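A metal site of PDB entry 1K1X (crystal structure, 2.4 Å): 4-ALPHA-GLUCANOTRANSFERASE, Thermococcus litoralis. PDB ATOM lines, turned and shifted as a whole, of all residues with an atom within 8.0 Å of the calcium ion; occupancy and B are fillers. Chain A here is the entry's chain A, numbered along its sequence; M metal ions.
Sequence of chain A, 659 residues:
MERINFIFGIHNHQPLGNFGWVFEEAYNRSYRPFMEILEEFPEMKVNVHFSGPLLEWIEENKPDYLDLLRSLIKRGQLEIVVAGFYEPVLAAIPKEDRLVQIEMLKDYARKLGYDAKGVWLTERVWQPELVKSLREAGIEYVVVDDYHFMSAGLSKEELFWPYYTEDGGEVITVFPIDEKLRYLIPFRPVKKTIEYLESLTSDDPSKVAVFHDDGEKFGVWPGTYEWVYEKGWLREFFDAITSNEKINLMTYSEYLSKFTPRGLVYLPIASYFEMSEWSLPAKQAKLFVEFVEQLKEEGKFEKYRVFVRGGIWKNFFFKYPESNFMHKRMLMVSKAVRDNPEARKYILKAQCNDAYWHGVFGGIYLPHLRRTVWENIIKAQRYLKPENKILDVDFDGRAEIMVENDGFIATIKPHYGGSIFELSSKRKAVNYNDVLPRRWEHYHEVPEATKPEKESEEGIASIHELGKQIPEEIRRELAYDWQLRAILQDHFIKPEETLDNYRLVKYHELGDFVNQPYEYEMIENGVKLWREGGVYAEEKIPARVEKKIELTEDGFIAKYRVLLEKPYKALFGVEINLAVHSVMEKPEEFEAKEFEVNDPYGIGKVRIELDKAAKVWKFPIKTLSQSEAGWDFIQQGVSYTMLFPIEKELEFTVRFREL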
ATOM      1  N   ASN A 324      18.765   4.481   0.260  1.00  0.00           N
ATOM      2  CA  ASN A 324      20.000   4.548  -0.517  1.00  0.00           C
ATOM      3  C   ASN A 324      20.472   6.013  -0.624  1.00  0.00           C
ATOM      4  O   ASN A 324      21.644   6.318  -0.396  1.00  0.00           O
ATOM      5  CB  ASN A 324      19.778   3.966  -1.913  1.00  0.00           C
ATOM      6  CG  ASN A 324      21.037   4.031  -2.759  1.00  0.00           C
ATOM      7  OD1 ASN A 324      22.105   3.611  -2.326  1.00  0.00           O
ATOM      8  ND2 ASN A 324      20.913   4.551  -3.969  1.00  0.00           N
ATOM      9  N   PHE A 325      19.531   6.889  -0.970  1.00  0.00           N
ATOM     10  CA  PHE A 325      19.861   8.303  -1.099  1.00  0.00           C
ATOM     11  C   PHE A 325      20.454   8.810   0.225  1.00  0.00           C
ATOM     12  O   PHE A 325      21.515   9.432   0.253  1.00  0.00           O
ATOM     13  CB  PHE A 325      18.596   9.098  -1.448  1.00  0.00           C
ATOM     14  CG  PHE A 325      18.857  10.556  -1.674  1.00  0.00           C
ATOM     15  CD1 PHE A 325      19.730  10.966  -2.665  1.00  0.00           C
ATOM     16  CD2 PHE A 325      18.272  11.507  -0.850  1.00  0.00           C
ATOM     17  CE1 PHE A 325      20.005  12.312  -2.855  1.00  0.00           C
ATOM     18  CE2 PHE A 325      18.543  12.861  -1.028  1.00  0.00           C
ATOM     19  CZ  PHE A 325      19.421  13.263  -2.031  1.00  0.00           C
ATOM     20  N   LEU A 391      26.588  15.703  -9.837  1.00  0.00           N
ATOM     21  CA  LEU A 391      27.168  14.378  -9.672  1.00  0.00           C
ATOM     22  C   LEU A 391      26.113  13.326  -9.389  1.00  0.00           C
ATOM     23  O   LEU A 391      25.004  13.646  -8.944  1.00  0.00           O
ATOM     24  CB  LEU A 391      28.184  14.373  -8.521  1.00  0.00           C
ATOM     25  CG  LEU A 391      27.592  14.422  -7.109  1.00  0.00           C
ATOM     26  CD1 LEU A 391      28.652  14.011  -6.101  1.00  0.00           C
ATOM     27  CD2 LEU A 391      27.039  15.803  -6.797  1.00  0.00           C
ATOM     28  N   ASP A 392      26.461  12.077  -9.673  1.00  0.00           N
ATOM     29  CA  ASP A 392      25.548  10.969  -9.433  1.00  0.00           C
ATOM     30  C   ASP A 392      25.683  10.578  -7.958  1.00  0.00           C
ATOM     31  O   ASP A 392      26.618   9.886  -7.566  1.00  0.00           O
ATOM     32  CB  ASP A 392      25.906   9.776 -10.307  1.00  0.00           C
ATOM     33  CG  ASP A 392      24.882   8.672 -10.221  1.00  0.00           C
ATOM     34  OD1 ASP A 392      24.203   8.607  -9.182  1.00  0.00           O
ATOM     35  OD2 ASP A 392      24.757   7.869 -11.177  1.00  0.00           O
ATOM     36  N   VAL A 393      24.741  11.044  -7.134  1.00  0.00           N
ATOM     37  CA  VAL A 393      24.786  10.756  -5.706  1.00  0.00           C
ATOM     38  C   VAL A 393      24.371   9.339  -5.331  1.00  0.00           C
ATOM     39  O   VAL A 393      25.084   8.658  -4.601  1.00  0.00           O
ATOM     40  CB  VAL A 393      23.897  11.769  -4.916  1.00  0.00           C
ATOM     41  CG1 VAL A 393      23.721  11.305  -3.470  1.00  0.00           C
ATOM     42  CG2 VAL A 393      24.556  13.147  -4.944  1.00  0.00           C
ATOM     43  N   ASP A 394      23.220   8.883  -5.823  1.00  0.00           N
ATOM     44  CA  ASP A 394      22.716   7.558  -5.496  1.00  0.00           C
ATOM     45  C   ASP A 394      23.064   6.451  -6.505  1.00  0.00           C
ATOM     46  O   ASP A 394      22.454   5.382  -6.509  1.00  0.00           O
ATOM     47  CB  ASP A 394      21.199   7.635  -5.319  1.00  0.00           C
ATOM     48  CG  ASP A 394      20.514   8.222  -6.529  1.00  0.00           C
ATOM     49  OD1 ASP A 394      19.269   8.308  -6.563  1.00  0.00           O
ATOM     50  OD2 ASP A 394      21.229   8.593  -7.466  1.00  0.00           O
ATOM     51  N   PHE A 395      24.050   6.725  -7.353  1.00  0.00           N
ATOM     52  CA  PHE A 395      24.538   5.776  -8.359  1.00  0.00           C
ATOM     53  C   PHE A 395      23.523   5.088  -9.262  1.00  0.00           C
ATOM     54  O   PHE A 395      23.478   3.857  -9.336  1.00  0.00           O
ATOM     55  CB  PHE A 395      25.386   4.691  -7.686  1.00  0.00           C
ATOM     56  CG  PHE A 395      26.491   5.238  -6.831  1.00  0.00           C
ATOM     57  CD1 PHE A 395      26.506   5.016  -5.461  1.00  0.00           C
ATOM     58  CD2 PHE A 395      27.517   5.980  -7.401  1.00  0.00           C
ATOM     59  CE1 PHE A 395      27.520   5.522  -4.655  1.00  0.00           C
ATOM     60  CE2 PHE A 395      28.549   6.489  -6.608  1.00  0.00           C
ATOM     61  CZ  PHE A 395      28.545   6.263  -5.225  1.00  0.00           C
ATOM     62  N   ASP A 396      22.718   5.864  -9.970  1.00  0.00           N
ATOM     63  CA  ASP A 396      21.745   5.285 -10.890  1.00  0.00           C
ATOM     64  C   ASP A 396      22.079   5.679 -12.326  1.00  0.00           C
ATOM     65  O   ASP A 396      21.297   5.429 -13.263  1.00  0.00           O
ATOM     66  CB  ASP A 396      20.306   5.700 -10.532  1.00  0.00           C
ATOM     67  CG  ASP A 396      20.095   7.200 -10.610  1.00  0.00           C
ATOM     68  OD1 ASP A 396      21.042   7.936 -10.967  1.00  0.00           O
ATOM     69  OD2 ASP A 396      18.971   7.653 -10.325  1.00  0.00           O
ATOM     70  N   GLY A 397      23.241   6.306 -12.511  1.00  0.00           N
ATOM     71  CA  GLY A 397      23.687   6.715 -13.833  1.00  0.00           C
ATOM     72  C   GLY A 397      23.085   7.992 -14.376  1.00  0.00           C
ATOM     73  O   GLY A 397      23.092   8.217 -15.593  1.00  0.00           O
ATOM     74  N   ARG A 398      22.550   8.837 -13.495  1.00  0.00           N
ATOM     75  CA  ARG A 398      21.940  10.093 -13.918  1.00  0.00           C
ATOM     76  C   ARG A 398      22.218  11.152 -12.856  1.00  0.00           C
ATOM     77  O   ARG A 398      21.537  11.219 -11.853  1.00  0.00           O
ATOM     78  CB  ARG A 398      20.442   9.887 -14.090  1.00  0.00           C
ATOM     79  CG  ARG A 398      20.105   8.624 -14.887  1.00  0.00           C
ATOM     80  CD  ARG A 398      19.484   8.946 -16.227  1.00  0.00           C
ATOM     81  NE  ARG A 398      18.040   9.126 -16.123  1.00  0.00           N
ATOM     82  CZ  ARG A 398      17.234   9.383 -17.148  1.00  0.00           C
ATOM     83  NH1 ARG A 398      17.744   9.492 -18.375  1.00  0.00           N
ATOM     84  NH2 ARG A 398      15.935   9.526 -16.962  1.00  0.00           N
ATOM     85  N   ALA A 399      23.222  11.988 -13.107  1.00  0.00           N
ATOM     86  CA  ALA A 399      23.625  13.043 -12.176  1.00  0.00           C
ATOM     87  C   ALA A 399      22.524  13.856 -11.476  1.00  0.00           C
ATOM     88  O   ALA A 399      21.473  14.147 -12.052  1.00  0.00           O
ATOM     89  CB  ALA A 399      24.602  13.990 -12.871  1.00  0.00           C
ATOM     90  N   GLU A 400      22.809  14.198 -10.227  1.00  0.00           N
ATOM     91  CA  GLU A 400      21.905  15.022  -9.426  1.00  0.00           C
ATOM     92  C   GLU A 400      22.500  16.424  -9.435  1.00  0.00           C
ATOM     93  O   GLU A 400      23.688  16.591  -9.717  1.00  0.00           O
ATOM     94  CB  GLU A 400      21.868  14.557  -7.962  1.00  0.00           C
ATOM     95  CG  GLU A 400      20.889  13.456  -7.639  1.00  0.00           C
ATOM     96  CD  GLU A 400      21.225  12.153  -8.320  1.00  0.00           C
ATOM     97  OE1 GLU A 400      22.338  11.614  -8.105  1.00  0.00           O
ATOM     98  OE2 GLU A 400      20.361  11.636  -9.068  1.00  0.00           O
ATOM     99  N   ILE A 401      21.673  17.418  -9.133  1.00  0.00           N
ATOM    100  CA  ILE A 401      22.173  18.780  -9.077  1.00  0.00           C
ATOM    101  C   ILE A 401      21.974  19.246  -7.639  1.00  0.00           C
ATOM    102  O   ILE A 401      20.856  19.216  -7.117  1.00  0.00           O
ATOM    103  CB  ILE A 401      21.385  19.744  -9.996  1.00  0.00           C
ATOM    104  CG1 ILE A 401      21.316  19.184 -11.419  1.00  0.00           C
ATOM    105  CG2 ILE A 401      22.074  21.105  -9.998  1.00  0.00           C
ATOM    106  CD1 ILE A 401      20.571  20.099 -12.386  1.00  0.00           C
ATOM    107  N   ILE A 412      18.316  18.228  -6.762  1.00  0.00           N
ATOM    108  CA  ILE A 412      17.377  18.095  -7.849  1.00  0.00           C
ATOM    109  C   ILE A 412      17.691  16.916  -8.743  1.00  0.00           C
ATOM    110  O   ILE A 412      18.857  16.630  -9.030  1.00  0.00           O
ATOM    111  CB  ILE A 412      17.367  19.382  -8.694  1.00  0.00           C
ATOM    112  CG1 ILE A 412      16.942  20.558  -7.803  1.00  0.00           C
ATOM    113  CG2 ILE A 412      16.433  19.228  -9.902  1.00  0.00           C
ATOM    114  CD1 ILE A 412      17.108  21.904  -8.453  1.00  0.00           C
ATOM    115  N   LYS A 413      16.645  16.224  -9.182  1.00  0.00           N
ATOM    116  CA  LYS A 413      16.807  15.093 -10.078  1.00  0.00           C
ATOM    117  C   LYS A 413      16.171  15.423 -11.412  1.00  0.00           C
ATOM    118  O   LYS A 413      14.957  15.309 -11.588  1.00  0.00           O
ATOM    119  CB  LYS A 413      16.174  13.838  -9.474  1.00  0.00           C
ATOM    120  CG  LYS A 413      17.035  13.197  -8.393  1.00  0.00           C
ATOM    121  CD  LYS A 413      16.399  11.946  -7.802  1.00  0.00           C
ATOM    122  CE  LYS A 413      17.399  11.203  -6.917  1.00  0.00           C
ATOM    123  NZ  LYS A 413      16.793  10.038  -6.216  1.00  0.00           N
ATOM    124  N   PRO A 414      16.988  15.886 -12.373  1.00  0.00           N
ATOM    125  CA  PRO A 414      16.482  16.241 -13.711  1.00  0.00           C
ATOM    126  C   PRO A 414      15.789  15.039 -14.337  1.00  0.00           C
ATOM    127  O   PRO A 414      14.691  15.155 -14.881  1.00  0.00           O
ATOM    128  CB  PRO A 414      17.749  16.633 -14.464  1.00  0.00           C
ATOM    129  CG  PRO A 414      18.608  17.217 -13.371  1.00  0.00           C
ATOM    130  CD  PRO A 414      18.409  16.234 -12.242  1.00  0.00           C
ATOM    131  N   HIS A 415      16.431  13.881 -14.257  1.00  0.00           N
ATOM    132  CA  HIS A 415      15.866  12.658 -14.829  1.00  0.00           C
ATOM    133  C   HIS A 415      14.490  12.268 -14.300  1.00  0.00           C
ATOM    134  O   HIS A 415      13.749  11.536 -14.956  1.00  0.00           O
ATOM    135  CB  HIS A 415      16.845  11.487 -14.659  1.00  0.00           C
ATOM    136  CG  HIS A 415      17.439  11.383 -13.287  1.00  0.00           C
ATOM    137  ND1 HIS A 415      18.261  12.366 -12.754  1.00  0.00           N
ATOM    138  CD2 HIS A 415      17.354  10.421 -12.348  1.00  0.00           C
ATOM    139  CE1 HIS A 415      18.651  11.998 -11.543  1.00  0.00           C
ATOM    140  NE2 HIS A 415      18.114  10.821 -11.277  1.00  0.00           N
HETATM  141 CA    CA M   1      21.815   9.573  -9.803  1.00  0.00          CA
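The calcium ion is bound by the side-chain carboxylate (OD1) of Asp 396 (2.2 Å), the side-chain carboxylate (OD2) of Asp 394 (2.6 Å), the side-chain carboxylate (OE2) of Glu 400 (2.6 Å), the backbone carbonyl oxygen (O) of Arg 398 (2.6 Å), the side-chain carboxylate (OD1) of Asp 392 (2.6 Å) and the side-chain carboxylate (OE1) of Glu 400 (2.7 Å).
Five residues have an atom within 4 Å of the calcium ion: Asp 392, Asp 394, Asp 396, Arg 398 and Glu 400.
Along chain A the residues within 4 Å of the calcium ion span positions 392 to 400.
The backbone NH (N) of Gly 397 lies within hydrogen-bond range of the side-chain carboxylate (OD2) of Asp 392, 2.6 Å away.
The backbone NH (N) of Glu 400 sits at hydrogen-bond distance from the backbone carbonyl oxygen (O) of Leu 391.
OE2 of Glu 400 lies close to NE2 of His 415 (3.3 Å).
N of Phe 395 sits close to OD1 of Asp 392.
The backbone carbonyl oxygen (O) of Asp 394 is in hydrogen-bond range of the side-chain amide nitrogen (ND2) of Asn 324 (3.1 Å).
NE2 of His 415 sits close to O of Arg 398 (3.5 Å).
The side-chain carboxylate (OD1) of Asp 394 is in salt-bridge range of the side-chain amino group (NZ) of Lys 413 (3.0 Å).
The side-chain carboxylate (OD2) of Asp 396 is in hydrogen-bond range of a ring nitrogen (NE2) of His 415, 3.4 Å away.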
